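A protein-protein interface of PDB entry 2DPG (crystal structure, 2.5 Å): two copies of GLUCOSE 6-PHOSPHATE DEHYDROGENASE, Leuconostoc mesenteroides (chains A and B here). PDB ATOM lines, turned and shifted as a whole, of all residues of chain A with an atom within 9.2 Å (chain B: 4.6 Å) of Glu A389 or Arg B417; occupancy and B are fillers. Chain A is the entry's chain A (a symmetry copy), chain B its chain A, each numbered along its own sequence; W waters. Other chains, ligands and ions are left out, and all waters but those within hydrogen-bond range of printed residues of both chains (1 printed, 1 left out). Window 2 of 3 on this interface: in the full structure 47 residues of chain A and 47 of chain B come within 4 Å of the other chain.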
ATOM      1  N   SER A 360      12.940  -9.656  -5.347  1.00  0.00           N
ATOM      2  CA  SER A 360      12.545  -9.839  -6.736  1.00  0.00           C
ATOM      3  C   SER A 360      12.037 -11.254  -6.985  1.00  0.00           C
ATOM      4  O   SER A 360      12.158 -12.120  -6.122  1.00  0.00           O
ATOM      5  CB  SER A 360      13.754  -9.568  -7.629  1.00  0.00           C
ATOM      6  OG  SER A 360      14.911 -10.202  -7.104  1.00  0.00           O
ATOM      7  N   GLU A 361      11.460 -11.479  -8.163  1.00  0.00           N
ATOM      8  CA  GLU A 361      10.956 -12.794  -8.551  1.00  0.00           C
ATOM      9  C   GLU A 361      12.119 -13.759  -8.622  1.00  0.00           C
ATOM     10  O   GLU A 361      12.031 -14.886  -8.148  1.00  0.00           O
ATOM     11  CB  GLU A 361      10.288 -12.743  -9.924  1.00  0.00           C
ATOM     12  CG  GLU A 361       8.802 -12.420  -9.892  1.00  0.00           C
ATOM     13  CD  GLU A 361       8.176 -12.412 -11.287  1.00  0.00           C
ATOM     14  OE1 GLU A 361       8.211 -13.468 -11.973  1.00  0.00           O
ATOM     15  OE2 GLU A 361       7.654 -11.345 -11.695  1.00  0.00           O
ATOM     16  N   GLN A 362      13.206 -13.308  -9.233  1.00  0.00           N
ATOM     17  CA  GLN A 362      14.406 -14.116  -9.379  1.00  0.00           C
ATOM     18  C   GLN A 362      15.480 -13.634  -8.408  1.00  0.00           C
ATOM     19  O   GLN A 362      15.946 -12.497  -8.494  1.00  0.00           O
ATOM     20  CB  GLN A 362      14.923 -14.038 -10.815  1.00  0.00           C
ATOM     21  CG  GLN A 362      16.126 -14.926 -11.094  1.00  0.00           C
ATOM     22  CD  GLN A 362      15.864 -16.386 -10.765  1.00  0.00           C
ATOM     23  OE1 GLN A 362      16.208 -16.858  -9.682  1.00  0.00           O
ATOM     24  NE2 GLN A 362      15.236 -17.103 -11.692  1.00  0.00           N
ATOM     25  N   ALA A 385      23.476 -10.287 -12.548  1.00  0.00           N
ATOM     26  CA  ALA A 385      23.349  -8.881 -12.918  1.00  0.00           C
ATOM     27  C   ALA A 385      21.867  -8.520 -12.870  1.00  0.00           C
ATOM     28  O   ALA A 385      21.056  -9.330 -12.425  1.00  0.00           O
ATOM     29  CB  ALA A 385      23.900  -8.668 -14.319  1.00  0.00           C
ATOM     30  N   LYS A 386      21.511  -7.308 -13.288  1.00  0.00           N
ATOM     31  CA  LYS A 386      20.110  -6.875 -13.300  1.00  0.00           C
ATOM     32  C   LYS A 386      19.482  -7.178 -14.658  1.00  0.00           C
ATOM     33  O   LYS A 386      20.098  -6.924 -15.702  1.00  0.00           O
ATOM     34  CB  LYS A 386      19.988  -5.371 -13.020  1.00  0.00           C
ATOM     35  CG  LYS A 386      18.559  -4.842 -13.186  1.00  0.00           C
ATOM     36  CD  LYS A 386      18.471  -3.336 -13.002  1.00  0.00           C
ATOM     37  CE  LYS A 386      17.020  -2.873 -13.048  1.00  0.00           C
ATOM     38  NZ  LYS A 386      16.380  -3.074 -14.385  1.00  0.00           N
ATOM     39  N   SER A 387      18.252  -7.682 -14.651  1.00  0.00           N
ATOM     40  CA  SER A 387      17.569  -7.991 -15.899  1.00  0.00           C
ATOM     41  C   SER A 387      17.002  -6.715 -16.501  1.00  0.00           C
ATOM     42  O   SER A 387      16.832  -5.708 -15.805  1.00  0.00           O
ATOM     43  CB  SER A 387      16.443  -8.988 -15.660  1.00  0.00           C
ATOM     44  OG  SER A 387      15.470  -8.447 -14.792  1.00  0.00           O
ATOM     45  N   VAL A 388      16.713  -6.763 -17.797  1.00  0.00           N
ATOM     46  CA  VAL A 388      16.160  -5.617 -18.496  1.00  0.00           C
ATOM     47  C   VAL A 388      14.642  -5.711 -18.412  1.00  0.00           C
ATOM     48  O   VAL A 388      13.986  -6.160 -19.348  1.00  0.00           O
ATOM     49  CB  VAL A 388      16.590  -5.604 -19.981  1.00  0.00           C
ATOM     50  CG1 VAL A 388      16.262  -4.270 -20.609  1.00  0.00           C
ATOM     51  CG2 VAL A 388      18.068  -5.915 -20.109  1.00  0.00           C
ATOM     52  N   GLU A 389      14.090  -5.354 -17.261  1.00  0.00           N
ATOM     53  CA  GLU A 389      12.648  -5.397 -17.066  1.00  0.00           C
ATOM     54  C   GLU A 389      12.198  -4.106 -16.423  1.00  0.00           C
ATOM     55  O   GLU A 389      13.012  -3.232 -16.141  1.00  0.00           O
ATOM     56  CB  GLU A 389      12.267  -6.571 -16.171  1.00  0.00           C
ATOM     57  CG  GLU A 389      12.535  -7.922 -16.786  1.00  0.00           C
ATOM     58  CD  GLU A 389      12.179  -9.062 -15.856  1.00  0.00           C
ATOM     59  OE1 GLU A 389      10.972  -9.343 -15.694  1.00  0.00           O
ATOM     60  OE2 GLU A 389      13.100  -9.683 -15.294  1.00  0.00           O
ATOM     61  N   ASP A 390      10.896  -3.984 -16.199  1.00  0.00           N
ATOM     62  CA  ASP A 390      10.358  -2.782 -15.570  1.00  0.00           C
ATOM     63  C   ASP A 390      10.586  -2.820 -14.061  1.00  0.00           C
ATOM     64  O   ASP A 390      10.857  -1.796 -13.443  1.00  0.00           O
ATOM     65  CB  ASP A 390       8.867  -2.605 -15.892  1.00  0.00           C
ATOM     66  CG  ASP A 390       8.613  -2.323 -17.366  1.00  0.00           C
ATOM     67  OD1 ASP A 390       9.439  -1.633 -17.997  1.00  0.00           O
ATOM     68  OD2 ASP A 390       7.584  -2.785 -17.900  1.00  0.00           O
ATOM     69  N   ALA A 391      10.480  -4.003 -13.467  1.00  0.00           N
ATOM     70  CA  ALA A 391      10.695  -4.152 -12.026  1.00  0.00           C
ATOM     71  C   ALA A 391      12.082  -4.706 -11.801  1.00  0.00           C
ATOM     72  O   ALA A 391      12.575  -5.484 -12.617  1.00  0.00           O
ATOM     73  CB  ALA A 391       9.664  -5.084 -11.425  1.00  0.00           C
ATOM     74  N   PHE A 392      12.712  -4.324 -10.697  1.00  0.00           N
ATOM     75  CA  PHE A 392      14.052  -4.816 -10.418  1.00  0.00           C
ATOM     76  C   PHE A 392      14.036  -6.334 -10.287  1.00  0.00           C
ATOM     77  O   PHE A 392      13.234  -6.891  -9.531  1.00  0.00           O
ATOM     78  CB  PHE A 392      14.611  -4.205  -9.135  1.00  0.00           C
ATOM     79  CG  PHE A 392      16.071  -4.487  -8.927  1.00  0.00           C
ATOM     80  CD1 PHE A 392      16.491  -5.656  -8.294  1.00  0.00           C
ATOM     81  CD2 PHE A 392      17.028  -3.602  -9.395  1.00  0.00           C
ATOM     82  CE1 PHE A 392      17.844  -5.937  -8.137  1.00  0.00           C
ATOM     83  CE2 PHE A 392      18.387  -3.873  -9.242  1.00  0.00           C
ATOM     84  CZ  PHE A 392      18.794  -5.041  -8.613  1.00  0.00           C
ATOM     85  N   ASN A 393      14.921  -6.994 -11.027  1.00  0.00           N
ATOM     86  CA  ASN A 393      15.017  -8.444 -10.997  1.00  0.00           C
ATOM     87  C   ASN A 393      16.429  -8.833 -11.392  1.00  0.00           C
ATOM     88  O   ASN A 393      17.146  -8.040 -12.000  1.00  0.00           O
ATOM     89  CB  ASN A 393      14.011  -9.057 -11.978  1.00  0.00           C
ATOM     90  CG  ASN A 393      13.727 -10.522 -11.682  1.00  0.00           C
ATOM     91  OD1 ASN A 393      13.828 -10.963 -10.542  1.00  0.00           O
ATOM     92  ND2 ASN A 393      13.340 -11.271 -12.698  1.00  0.00           N
ATOM     93  N   THR A 394      16.847 -10.037 -11.022  1.00  0.00           N
ATOM     94  CA  THR A 394      18.181 -10.500 -11.373  1.00  0.00           C
ATOM     95  C   THR A 394      18.115 -11.464 -12.558  1.00  0.00           C
ATOM     96  O   THR A 394      17.041 -11.945 -12.937  1.00  0.00           O
ATOM     97  CB  THR A 394      18.910 -11.191 -10.184  1.00  0.00           C
ATOM     98  OG1 THR A 394      18.267 -12.431  -9.875  1.00  0.00           O
ATOM     99  CG2 THR A 394      18.910 -10.297  -8.955  1.00  0.00           C
ATOM    100  N   ARG A 395      19.273 -11.701 -13.154  1.00  0.00           N
ATOM    101  CA  ARG A 395      19.430 -12.597 -14.286  1.00  0.00           C
ATOM    102  C   ARG A 395      20.907 -12.949 -14.219  1.00  0.00           C
ATOM    103  O   ARG A 395      21.654 -12.328 -13.454  1.00  0.00           O
ATOM    104  CB  ARG A 395      19.144 -11.855 -15.606  1.00  0.00           C
ATOM    105  CG  ARG A 395      20.368 -11.128 -16.179  1.00  0.00           C
ATOM    106  CD  ARG A 395      20.049  -9.826 -16.855  1.00  0.00           C
ATOM    107  NE  ARG A 395      19.793  -9.957 -18.279  1.00  0.00           N
ATOM    108  CZ  ARG A 395      20.201  -9.077 -19.194  1.00  0.00           C
ATOM    109  NH1 ARG A 395      20.903  -8.005 -18.846  1.00  0.00           N
ATOM    110  NH2 ARG A 395      19.839  -9.229 -20.464  1.00  0.00           N
ATOM    111  N   GLY B 181      18.889   7.151 -13.334  1.00  0.00           N
ATOM    112  CA  GLY B 181      17.876   6.394 -14.042  1.00  0.00           C
ATOM    113  C   GLY B 181      18.423   5.563 -15.191  1.00  0.00           C
ATOM    114  O   GLY B 181      17.657   5.128 -16.056  1.00  0.00           O
ATOM    115  N   GLU B 183      20.178   2.230 -16.851  1.00  0.00           N
ATOM    116  CA  GLU B 183      20.196   0.782 -16.670  1.00  0.00           C
ATOM    117  C   GLU B 183      21.489   0.238 -16.043  1.00  0.00           C
ATOM    118  O   GLU B 183      21.441  -0.466 -15.033  1.00  0.00           O
ATOM    119  CB  GLU B 183      19.944   0.106 -18.023  1.00  0.00           C
ATOM    120  CG  GLU B 183      19.507  -1.347 -17.952  1.00  0.00           C
ATOM    121  CD  GLU B 183      18.109  -1.519 -17.386  1.00  0.00           C
ATOM    122  OE1 GLU B 183      17.122  -1.265 -18.110  1.00  0.00           O
ATOM    123  OE2 GLU B 183      17.994  -1.931 -16.219  1.00  0.00           O
ATOM    124  N   GLN B 186      22.091   1.010 -12.468  1.00  0.00           N
ATOM    125  CA  GLN B 186      21.253   0.178 -11.628  1.00  0.00           C
ATOM    126  C   GLN B 186      21.749  -1.260 -11.518  1.00  0.00           C
ATOM    127  O   GLN B 186      21.243  -2.034 -10.705  1.00  0.00           O
ATOM    128  CB  GLN B 186      19.822   0.233 -12.125  1.00  0.00           C
ATOM    129  CG  GLN B 186      19.201   1.588 -11.868  1.00  0.00           C
ATOM    130  CD  GLN B 186      17.836   1.755 -12.496  1.00  0.00           C
ATOM    131  OE1 GLN B 186      17.024   0.823 -12.538  1.00  0.00           O
ATOM    132  NE2 GLN B 186      17.563   2.964 -12.964  1.00  0.00           N
ATOM    133  N   PRO B 412      13.634   0.481 -20.688  1.00  0.00           N
ATOM    134  CA  PRO B 412      12.699   1.610 -20.572  1.00  0.00           C
ATOM    135  C   PRO B 412      13.433   2.948 -20.697  1.00  0.00           C
ATOM    136  O   PRO B 412      14.581   3.077 -20.266  1.00  0.00           O
ATOM    137  CB  PRO B 412      12.134   1.445 -19.157  1.00  0.00           C
ATOM    138  CG  PRO B 412      12.299  -0.018 -18.873  1.00  0.00           C
ATOM    139  CD  PRO B 412      13.659  -0.302 -19.443  1.00  0.00           C
ATOM    140  N   GLU B 413      12.778   3.935 -21.303  1.00  0.00           N
ATOM    141  CA  GLU B 413      13.370   5.264 -21.460  1.00  0.00           C
ATOM    142  C   GLU B 413      13.614   5.878 -20.086  1.00  0.00           C
ATOM    143  O   GLU B 413      12.817   5.677 -19.167  1.00  0.00           O
ATOM    144  CB  GLU B 413      12.433   6.169 -22.257  1.00  0.00           C
ATOM    145  CG  GLU B 413      12.382   5.865 -23.739  1.00  0.00           C
ATOM    146  CD  GLU B 413      13.526   6.506 -24.502  1.00  0.00           C
ATOM    147  OE1 GLU B 413      14.700   6.143 -24.253  1.00  0.00           O
ATOM    148  OE2 GLU B 413      13.242   7.386 -25.347  1.00  0.00           O
ATOM    149  N   PRO B 414      14.671   6.694 -19.949  1.00  0.00           N
ATOM    150  CA  PRO B 414      15.000   7.335 -18.671  1.00  0.00           C
ATOM    151  C   PRO B 414      13.812   8.035 -17.994  1.00  0.00           C
ATOM    152  O   PRO B 414      13.605   7.890 -16.785  1.00  0.00           O
ATOM    153  CB  PRO B 414      16.112   8.313 -19.060  1.00  0.00           C
ATOM    154  CG  PRO B 414      15.841   8.584 -20.527  1.00  0.00           C
ATOM    155  CD  PRO B 414      15.532   7.210 -21.026  1.00  0.00           C
ATOM    156  N   TYR B 415      13.017   8.769 -18.768  1.00  0.00           N
ATOM    157  CA  TYR B 415      11.860   9.452 -18.197  1.00  0.00           C
ATOM    158  C   TYR B 415      10.714   8.500 -17.866  1.00  0.00           C
ATOM    159  O   TYR B 415       9.978   8.736 -16.904  1.00  0.00           O
ATOM    160  CB  TYR B 415      11.390  10.605 -19.090  1.00  0.00           C
ATOM    161  CG  TYR B 415      12.118  11.902 -18.797  1.00  0.00           C
ATOM    162  CD1 TYR B 415      11.885  12.605 -17.613  1.00  0.00           C
ATOM    163  CD2 TYR B 415      13.076  12.399 -19.676  1.00  0.00           C
ATOM    164  CE1 TYR B 415      12.589  13.763 -17.309  1.00  0.00           C
ATOM    165  CE2 TYR B 415      13.791  13.558 -19.384  1.00  0.00           C
ATOM    166  CZ  TYR B 415      13.542  14.230 -18.196  1.00  0.00           C
ATOM    167  OH  TYR B 415      14.282  15.350 -17.882  1.00  0.00           O
ATOM    168  N   GLU B 416      10.591   7.410 -18.626  1.00  0.00           N
ATOM    169  CA  GLU B 416       9.552   6.410 -18.378  1.00  0.00           C
ATOM    170  C   GLU B 416       9.834   5.798 -17.006  1.00  0.00           C
ATOM    171  O   GLU B 416       8.937   5.666 -16.159  1.00  0.00           O
ATOM    172  CB  GLU B 416       9.595   5.303 -19.435  1.00  0.00           C
ATOM    173  CG  GLU B 416       8.414   4.343 -19.352  1.00  0.00           C
ATOM    174  CD  GLU B 416       8.572   3.101 -20.216  1.00  0.00           C
ATOM    175  OE1 GLU B 416       8.986   3.212 -21.392  1.00  0.00           O
ATOM    176  OE2 GLU B 416       8.261   2.001 -19.713  1.00  0.00           O
ATOM    177  N   ARG B 417      11.106   5.470 -16.795  1.00  0.00           N
ATOM    178  CA  ARG B 417      11.588   4.891 -15.554  1.00  0.00           C
ATOM    179  C   ARG B 417      11.252   5.785 -14.366  1.00  0.00           C
ATOM    180  O   ARG B 417      10.633   5.336 -13.392  1.00  0.00           O
ATOM    181  CB  ARG B 417      13.109   4.719 -15.630  1.00  0.00           C
ATOM    182  CG  ARG B 417      13.564   3.370 -16.101  1.00  0.00           C
ATOM    183  CD  ARG B 417      14.065   2.553 -14.918  1.00  0.00           C
ATOM    184  NE  ARG B 417      14.101   1.120 -15.210  1.00  0.00           N
ATOM    185  CZ  ARG B 417      15.053   0.505 -15.912  1.00  0.00           C
ATOM    186  NH1 ARG B 417      16.078   1.188 -16.412  1.00  0.00           N
ATOM    187  NH2 ARG B 417      14.967  -0.805 -16.129  1.00  0.00           N
ATOM    188  N   MET B 418      11.641   7.057 -14.466  1.00  0.00           N
ATOM    189  CA  MET B 418      11.427   8.019 -13.396  1.00  0.00           C
ATOM    190  C   MET B 418       9.961   8.279 -13.064  1.00  0.00           C
ATOM    191  O   MET B 418       9.589   8.334 -11.884  1.00  0.00           O
ATOM    192  CB  MET B 418      12.161   9.322 -13.704  1.00  0.00           C
ATOM    193  CG  MET B 418      13.676   9.179 -13.672  1.00  0.00           C
ATOM    194  SD  MET B 418      14.524  10.755 -13.833  1.00  0.00           S
ATOM    195  CE  MET B 418      14.889  10.795 -15.569  1.00  0.00           C
ATOM    196  N   ILE B 419       9.127   8.417 -14.090  1.00  0.00           N
ATOM    197  CA  ILE B 419       7.706   8.647 -13.862  1.00  0.00           C
ATOM    198  C   ILE B 419       7.125   7.403 -13.186  1.00  0.00           C
ATOM    199  O   ILE B 419       6.398   7.495 -12.177  1.00  0.00           O
ATOM    200  CB  ILE B 419       6.945   8.879 -15.180  1.00  0.00           C
ATOM    201  CG1 ILE B 419       7.485  10.116 -15.901  1.00  0.00           C
ATOM    202  CG2 ILE B 419       5.451   9.029 -14.910  1.00  0.00           C
ATOM    203  CD1 ILE B 419       7.198  11.411 -15.202  1.00  0.00           C
ATOM    204  N   HIS B 420       7.494   6.242 -13.724  1.00  0.00           N
ATOM    205  CA  HIS B 420       7.021   4.970 -13.204  1.00  0.00           C
ATOM    206  C   HIS B 420       7.365   4.758 -11.726  1.00  0.00           C
ATOM    207  O   HIS B 420       6.494   4.381 -10.933  1.00  0.00           O
ATOM    208  CB  HIS B 420       7.583   3.832 -14.051  1.00  0.00           C
ATOM    209  CG  HIS B 420       6.841   2.540 -13.897  1.00  0.00           C
ATOM    210  ND1 HIS B 420       7.074   1.451 -14.711  1.00  0.00           N
ATOM    211  CD2 HIS B 420       5.871   2.159 -13.030  1.00  0.00           C
ATOM    212  CE1 HIS B 420       6.282   0.456 -14.356  1.00  0.00           C
ATOM    213  NE2 HIS B 420       5.542   0.857 -13.338  1.00  0.00           N
ATOM    214  N   ASP B 421       8.618   5.018 -11.355  1.00  0.00           N
ATOM    215  CA  ASP B 421       9.066   4.857  -9.973  1.00  0.00           C
ATOM    216  C   ASP B 421       8.356   5.799  -9.018  1.00  0.00           C
ATOM    217  O   ASP B 421       8.080   5.429  -7.876  1.00  0.00           O
ATOM    218  CB  ASP B 421      10.580   5.035  -9.866  1.00  0.00           C
ATOM    219  CG  ASP B 421      11.347   3.863 -10.452  1.00  0.00           C
ATOM    220  OD1 ASP B 421      10.770   2.756 -10.555  1.00  0.00           O
ATOM    221  OD2 ASP B 421      12.531   4.041 -10.804  1.00  0.00           O
HETATM  222  O   HOH W   1       8.407   1.141 -17.011  1.00  0.00           O
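NH2 of Arg B417 is in salt-bridge range of OE1 of Glu B183, 3.0 Å away.
The backbone carbonyl oxygen (O) of Lys A386 lies close to the guanidinium group (NH1) of Arg A395 (3.4 Å).
OE2 of Glu A389 sits at hydrogen-bond distance from OG of Ser A387 (2.7 Å).
N of Ser A387 is in hydrogen-bond range of O of Asn A393 (2.9 Å).
The side-chain amide nitrogen (ND2) of Asn A393 is in hydrogen-bond range of the side-chain carboxylate (OE2) of Glu A389 (3.1 Å).
The side-chain amino group of Lys A386 is in salt-bridge range of the side-chain carboxylate of Glu B183 (2.7 Å).
The guanidinium group of Arg B417 is in hydrogen-bond range of the backbone carbonyl oxygen of Glu A389, at 3.1 Å.
NH2 of Arg B417 sits close to NZ of Lys A386, 3.2 Å away.
Printed residues of chain B that touch a printed residue of chain A: Glu B183, Gln B186, Pro B412 and Arg B417.
Hydrophobic or aromatic side chains of chain B that line the printed part of chain A: Pro B412.
Of the 14 printed residues of chain A, 5 touch a printed residue of chain B.
Printed residues of chain A that touch a printed residue of chain B: Lys A386, Ser A387, Glu A389, Asp A390 and Phe A392.
Hydrophobic or aromatic side chains of chain A that line the printed part of chain B: Phe A392.
Among the printed residues, Asp or Glu carboxylates within 4 Å of a Lys or Arg side-chain nitrogen of the other chain: Lys A386 with Glu B183.
Among the printed residues, pairs that only touch across the chains: Asp A390 with Pro B412, Phe A392 with Gln B186, Lys A386 with Gln B186 and Ser A387 with Glu B183.
No position is printed for both chains.
Of the 7 pairs that touch across the chains among the printed residues, none has its exchanged pair printed and touching as well.
Water W1 lies within hydrogen-bond range of a ring nitrogen (ND1) of His B420, the side-chain carboxylate (OE2) of Glu B416 and the side-chain carboxylate (OD1) of Asp A390.
Printed residues of chain B within 4 Å of Lys A386: Glu B183 (2.7 Å), Gln B186 (3.7 Å) and Arg B417 (3.2 Å).
Of chain B, only Arg B417 (3.1 Å) comes within 4 Å of Glu A389.
Of the printed residues of chain B, Asp A390 touches Pro B412.
Of the printed residues of chain A, Glu B183 touches Lys A386 (2.7 Å) and Ser A387 (3.97 Å).
Printed residues of chain A within 4 Å of Gln B186: Lys A386 and Phe A392.
Pro B412 touches just one residue of chain A: Asp A390 (3.4 Å).
The nearest residue of chain B that does not touch Glu A389 is Pro B412 (4.3 Å).
The nearest residue of chain A that does not touch Arg B417 is Asp A390 (4.7 Å).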
